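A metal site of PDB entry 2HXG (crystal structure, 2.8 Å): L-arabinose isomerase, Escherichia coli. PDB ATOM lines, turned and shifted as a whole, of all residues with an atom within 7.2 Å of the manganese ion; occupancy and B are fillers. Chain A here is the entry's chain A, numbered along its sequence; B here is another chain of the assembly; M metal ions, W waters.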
ATOM      1  N   MET A 185     -24.720 -22.903 -11.431  1.00  0.00           N
ATOM      2  CA  MET A 185     -25.078 -22.614 -12.814  1.00  0.00           C
ATOM      3  C   MET A 185     -26.182 -23.616 -13.197  1.00  0.00           C
ATOM      4  O   MET A 185     -26.087 -24.826 -12.900  1.00  0.00           O
ATOM      5  CB  MET A 185     -23.851 -22.728 -13.731  1.00  0.00           C
ATOM      6  CG  MET A 185     -24.071 -22.255 -15.152  1.00  0.00           C
ATOM      7  SD  MET A 185     -22.705 -22.667 -16.289  1.00  0.00           S
ATOM      8  CE  MET A 185     -21.295 -22.296 -15.311  1.00  0.00           C
ATOM      9  N   PHE A 279     -22.430 -16.215 -12.254  1.00  0.00           N
ATOM     10  CA  PHE A 279     -22.678 -15.132 -13.210  1.00  0.00           C
ATOM     11  C   PHE A 279     -24.165 -14.972 -13.578  1.00  0.00           C
ATOM     12  O   PHE A 279     -24.584 -13.906 -14.039  1.00  0.00           O
ATOM     13  CB  PHE A 279     -21.818 -15.299 -14.470  1.00  0.00           C
ATOM     14  CG  PHE A 279     -22.031 -16.580 -15.198  1.00  0.00           C
ATOM     15  CD1 PHE A 279     -23.147 -16.769 -15.993  1.00  0.00           C
ATOM     16  CD2 PHE A 279     -21.096 -17.594 -15.113  1.00  0.00           C
ATOM     17  CE1 PHE A 279     -23.336 -17.965 -16.684  1.00  0.00           C
ATOM     18  CE2 PHE A 279     -21.274 -18.786 -15.796  1.00  0.00           C
ATOM     19  CZ  PHE A 279     -22.392 -18.974 -16.577  1.00  0.00           C
ATOM     20  N   GLY A 305     -15.767 -21.471  -9.116  1.00  0.00           N
ATOM     21  CA  GLY A 305     -16.666 -20.677  -9.947  1.00  0.00           C
ATOM     22  C   GLY A 305     -18.068 -21.220  -9.998  1.00  0.00           C
ATOM     23  O   GLY A 305     -18.327 -22.379  -9.672  1.00  0.00           O
ATOM     24  N   GLU A 306     -18.995 -20.354 -10.402  1.00  0.00           N
ATOM     25  CA  GLU A 306     -20.379 -20.727 -10.617  1.00  0.00           C
ATOM     26  C   GLU A 306     -20.851 -21.777  -9.626  1.00  0.00           C
ATOM     27  O   GLU A 306     -21.078 -22.931  -9.981  1.00  0.00           O
ATOM     28  CB  GLU A 306     -20.606 -21.177 -12.070  1.00  0.00           C
ATOM     29  CG  GLU A 306     -19.546 -22.148 -12.613  1.00  0.00           C
ATOM     30  CD  GLU A 306     -18.569 -21.551 -13.629  1.00  0.00           C
ATOM     31  OE1 GLU A 306     -17.596 -22.253 -13.991  1.00  0.00           O
ATOM     32  OE2 GLU A 306     -18.791 -20.416 -14.110  1.00  0.00           O
ATOM     33  N   PHE A 331      -7.540 -22.534  -7.794  1.00  0.00           N
ATOM     34  CA  PHE A 331      -8.683 -22.935  -8.595  1.00  0.00           C
ATOM     35  C   PHE A 331      -8.241 -22.969 -10.057  1.00  0.00           C
ATOM     36  O   PHE A 331      -7.354 -22.209 -10.458  1.00  0.00           O
ATOM     37  CB  PHE A 331      -9.850 -21.963  -8.380  1.00  0.00           C
ATOM     38  CG  PHE A 331     -11.065 -22.278  -9.204  1.00  0.00           C
ATOM     39  CD1 PHE A 331     -11.701 -23.496  -9.099  1.00  0.00           C
ATOM     40  CD2 PHE A 331     -11.580 -21.350 -10.082  1.00  0.00           C
ATOM     41  CE1 PHE A 331     -12.835 -23.787  -9.869  1.00  0.00           C
ATOM     42  CE2 PHE A 331     -12.720 -21.636 -10.847  1.00  0.00           C
ATOM     43  CZ  PHE A 331     -13.339 -22.856 -10.739  1.00  0.00           C
ATOM     44  N   MET A 332      -8.811 -23.882 -10.833  1.00  0.00           N
ATOM     45  CA  MET A 332      -8.372 -24.123 -12.204  1.00  0.00           C
ATOM     46  C   MET A 332      -9.414 -24.912 -12.980  1.00  0.00           C
ATOM     47  O   MET A 332     -10.098 -25.779 -12.416  1.00  0.00           O
ATOM     48  CB  MET A 332      -7.070 -24.924 -12.209  1.00  0.00           C
ATOM     49  CG  MET A 332      -6.434 -25.083 -13.594  1.00  0.00           C
ATOM     50  SD  MET A 332      -5.914 -23.513 -14.292  1.00  0.00           S
ATOM     51  CE  MET A 332      -4.566 -23.143 -13.200  1.00  0.00           C
ATOM     52  N   GLU A 333      -9.522 -24.626 -14.286  1.00  0.00           N
ATOM     53  CA  GLU A 333     -10.447 -25.329 -15.191  1.00  0.00           C
ATOM     54  C   GLU A 333      -9.814 -25.565 -16.559  1.00  0.00           C
ATOM     55  O   GLU A 333      -9.536 -24.616 -17.295  1.00  0.00           O
ATOM     56  CB  GLU A 333     -11.756 -24.548 -15.358  1.00  0.00           C
ATOM     57  CG  GLU A 333     -12.845 -25.297 -16.118  1.00  0.00           C
ATOM     58  CD  GLU A 333     -14.025 -24.414 -16.508  1.00  0.00           C
ATOM     59  OE1 GLU A 333     -13.779 -23.359 -17.112  1.00  0.00           O
ATOM     60  OE2 GLU A 333     -15.194 -24.764 -16.236  1.00  0.00           O
ATOM     61  N   TYR A 335      -9.153 -25.584 -20.010  1.00  0.00           N
ATOM     62  CA  TYR A 335      -9.841 -24.667 -20.916  1.00  0.00           C
ATOM     63  C   TYR A 335      -9.690 -25.044 -22.381  1.00  0.00           C
ATOM     64  O   TYR A 335     -10.662 -24.976 -23.113  1.00  0.00           O
ATOM     65  CB  TYR A 335      -9.456 -23.200 -20.683  1.00  0.00           C
ATOM     66  CG  TYR A 335     -10.699 -22.360 -20.499  1.00  0.00           C
ATOM     67  CD1 TYR A 335     -11.092 -21.920 -19.234  1.00  0.00           C
ATOM     68  CD2 TYR A 335     -11.544 -22.095 -21.569  1.00  0.00           C
ATOM     69  CE1 TYR A 335     -12.255 -21.188 -19.052  1.00  0.00           C
ATOM     70  CE2 TYR A 335     -12.727 -21.357 -21.399  1.00  0.00           C
ATOM     71  CZ  TYR A 335     -13.071 -20.907 -20.141  1.00  0.00           C
ATOM     72  OH  TYR A 335     -14.219 -20.174 -19.943  1.00  0.00           O
ATOM     73  N   SER A 349      -7.252 -22.397 -17.072  1.00  0.00           N
ATOM     74  CA  SER A 349      -7.618 -21.017 -16.721  1.00  0.00           C
ATOM     75  C   SER A 349      -9.059 -20.981 -16.197  1.00  0.00           C
ATOM     76  O   SER A 349      -9.671 -22.037 -16.022  1.00  0.00           O
ATOM     77  CB  SER A 349      -7.491 -20.079 -17.935  1.00  0.00           C
ATOM     78  OG  SER A 349      -8.030 -18.800 -17.650  1.00  0.00           O
ATOM     79  N   HIS A 350      -9.547 -19.785 -15.899  1.00  0.00           N
ATOM     80  CA  HIS A 350     -10.983 -19.567 -15.731  1.00  0.00           C
ATOM     81  C   HIS A 350     -11.363 -18.206 -16.312  1.00  0.00           C
ATOM     82  O   HIS A 350     -10.496 -17.365 -16.597  1.00  0.00           O
ATOM     83  CB  HIS A 350     -11.438 -19.692 -14.258  1.00  0.00           C
ATOM     84  CG  HIS A 350     -12.851 -20.188 -14.093  1.00  0.00           C
ATOM     85  ND1 HIS A 350     -13.809 -19.502 -13.387  1.00  0.00           N
ATOM     86  CD2 HIS A 350     -13.469 -21.312 -14.554  1.00  0.00           C
ATOM     87  CE1 HIS A 350     -14.951 -20.173 -13.408  1.00  0.00           C
ATOM     88  NE2 HIS A 350     -14.766 -21.279 -14.114  1.00  0.00           N
ATOM     89  N   MET A 351     -12.671 -18.041 -16.527  1.00  0.00           N
ATOM     90  CA  MET A 351     -13.298 -16.774 -16.919  1.00  0.00           C
ATOM     91  C   MET A 351     -12.479 -15.571 -16.465  1.00  0.00           C
ATOM     92  O   MET A 351     -12.079 -14.750 -17.279  1.00  0.00           O
ATOM     93  CB  MET A 351     -14.691 -16.780 -16.281  1.00  0.00           C
ATOM     94  CG  MET A 351     -15.682 -15.742 -16.746  1.00  0.00           C
ATOM     95  SD  MET A 351     -17.365 -16.350 -16.532  1.00  0.00           S
ATOM     96  CE  MET A 351     -17.217 -17.078 -14.910  1.00  0.00           C
ATOM     97  N   GLU A 353     -11.094 -16.041 -12.692  1.00  0.00           N
ATOM     98  CA  GLU A 353     -10.687 -16.345 -11.328  1.00  0.00           C
ATOM     99  C   GLU A 353      -9.584 -17.382 -11.299  1.00  0.00           C
ATOM    100  O   GLU A 353      -9.850 -18.585 -11.287  1.00  0.00           O
ATOM    101  CB  GLU A 353     -11.907 -16.826 -10.512  1.00  0.00           C
ATOM    102  CG  GLU A 353     -13.180 -15.984 -10.695  1.00  0.00           C
ATOM    103  CD  GLU A 353     -14.135 -16.503 -11.781  1.00  0.00           C
ATOM    104  OE1 GLU A 353     -15.355 -16.349 -11.627  1.00  0.00           O
ATOM    105  OE2 GLU A 353     -13.684 -17.072 -12.796  1.00  0.00           O
ATOM    106  N   HIS A 449     -14.630 -30.757 -14.447  1.00  0.00           N
ATOM    107  CA  HIS A 449     -13.884 -29.796 -15.231  1.00  0.00           C
ATOM    108  C   HIS A 449     -13.189 -28.794 -14.323  1.00  0.00           C
ATOM    109  O   HIS A 449     -12.155 -28.238 -14.680  1.00  0.00           O
ATOM    110  CB  HIS A 449     -14.794 -29.084 -16.233  1.00  0.00           C
ATOM    111  CG  HIS A 449     -16.013 -28.476 -15.610  1.00  0.00           C
ATOM    112  ND1 HIS A 449     -16.076 -27.157 -15.208  1.00  0.00           N
ATOM    113  CD2 HIS A 449     -17.232 -29.007 -15.330  1.00  0.00           C
ATOM    114  CE1 HIS A 449     -17.267 -26.900 -14.701  1.00  0.00           C
ATOM    115  NE2 HIS A 449     -17.988 -27.993 -14.763  1.00  0.00           N
ATOM    116  N   HIS A 450     -13.783 -28.563 -13.143  1.00  0.00           N
ATOM    117  CA  HIS A 450     -13.211 -27.707 -12.105  1.00  0.00           C
ATOM    118  C   HIS A 450     -12.227 -28.507 -11.261  1.00  0.00           C
ATOM    119  O   HIS A 450     -12.585 -29.557 -10.719  1.00  0.00           O
ATOM    120  CB  HIS A 450     -14.305 -27.169 -11.193  1.00  0.00           C
ATOM    121  CG  HIS A 450     -15.105 -26.042 -11.762  1.00  0.00           C
ATOM    122  ND1 HIS A 450     -16.205 -25.510 -11.124  1.00  0.00           N
ATOM    123  CD2 HIS A 450     -14.967 -25.350 -12.920  1.00  0.00           C
ATOM    124  CE1 HIS A 450     -16.706 -24.543 -11.861  1.00  0.00           C
ATOM    125  NE2 HIS A 450     -15.982 -24.413 -12.951  1.00  0.00           N
ATOM    126  N   PHE B  83     -19.042 -26.188 -23.563  1.00  0.00           N
ATOM    127  CA  PHE B  83     -19.663 -26.655 -22.332  1.00  0.00           C
ATOM    128  C   PHE B  83     -21.101 -26.969 -22.651  1.00  0.00           C
ATOM    129  O   PHE B  83     -21.709 -26.317 -23.494  1.00  0.00           O
ATOM    130  CB  PHE B  83     -19.586 -25.577 -21.254  1.00  0.00           C
ATOM    131  CG  PHE B  83     -19.808 -26.070 -19.839  1.00  0.00           C
ATOM    132  CD1 PHE B  83     -20.879 -25.602 -19.087  1.00  0.00           C
ATOM    133  CD2 PHE B  83     -18.922 -26.955 -19.244  1.00  0.00           C
ATOM    134  CE1 PHE B  83     -21.064 -26.033 -17.782  1.00  0.00           C
ATOM    135  CE2 PHE B  83     -19.105 -27.374 -17.948  1.00  0.00           C
ATOM    136  CZ  PHE B  83     -20.184 -26.913 -17.218  1.00  0.00           C
ATOM    137  N   HIS B 128     -13.047 -28.947 -21.216  1.00  0.00           N
ATOM    138  CA  HIS B 128     -13.857 -29.006 -20.005  1.00  0.00           C
ATOM    139  C   HIS B 128     -15.278 -29.478 -20.257  1.00  0.00           C
ATOM    140  O   HIS B 128     -15.841 -30.200 -19.439  1.00  0.00           O
ATOM    141  CB  HIS B 128     -13.824 -27.691 -19.175  1.00  0.00           C
ATOM    142  CG  HIS B 128     -14.384 -26.479 -19.838  1.00  0.00           C
ATOM    143  ND1 HIS B 128     -13.603 -25.433 -20.279  1.00  0.00           N
ATOM    144  CD2 HIS B 128     -15.669 -26.098 -20.056  1.00  0.00           C
ATOM    145  CE1 HIS B 128     -14.378 -24.485 -20.770  1.00  0.00           C
ATOM    146  NE2 HIS B 128     -15.639 -24.861 -20.654  1.00  0.00           N
HETATM  147 MN    MN M   1     -16.001 -22.914 -14.870  1.00  0.00          MN
HETATM  148  O   HOH W   1     -17.330 -21.917 -16.773  1.00  0.00           O
HETATM  149  O   HOH W   2     -17.725 -24.086 -16.619  1.00  0.00           O
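The side-chain carboxylate (OE2) of Glu 353 lies within hydrogen-bond range of a ring nitrogen (ND1) of His 350 (2.5 Å). The backbone NH of Glu 333 sits at hydrogen-bond distance from the backbone carbonyl oxygen of Ser 349, 3.1 Å away. OE2 of Glu 333 sits close to ND1 of His 449 (2.7 Å).
Of the 16 residues printed, 4 come within 4 Å of the manganese ion.
The manganese ion is bound by the side-chain carboxylate of Glu 306 (1.9 Å), a ring nitrogen (NE2) of His 350 (2.2 Å), a ring nitrogen (NE2) of His 450 (2.4 Å), the side-chain carboxylate of Glu 333 (2.4 Å), water W1 (2.5 Å) and water W2 (2.7 Å). The manganese ion has six donor atoms within binding distance.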
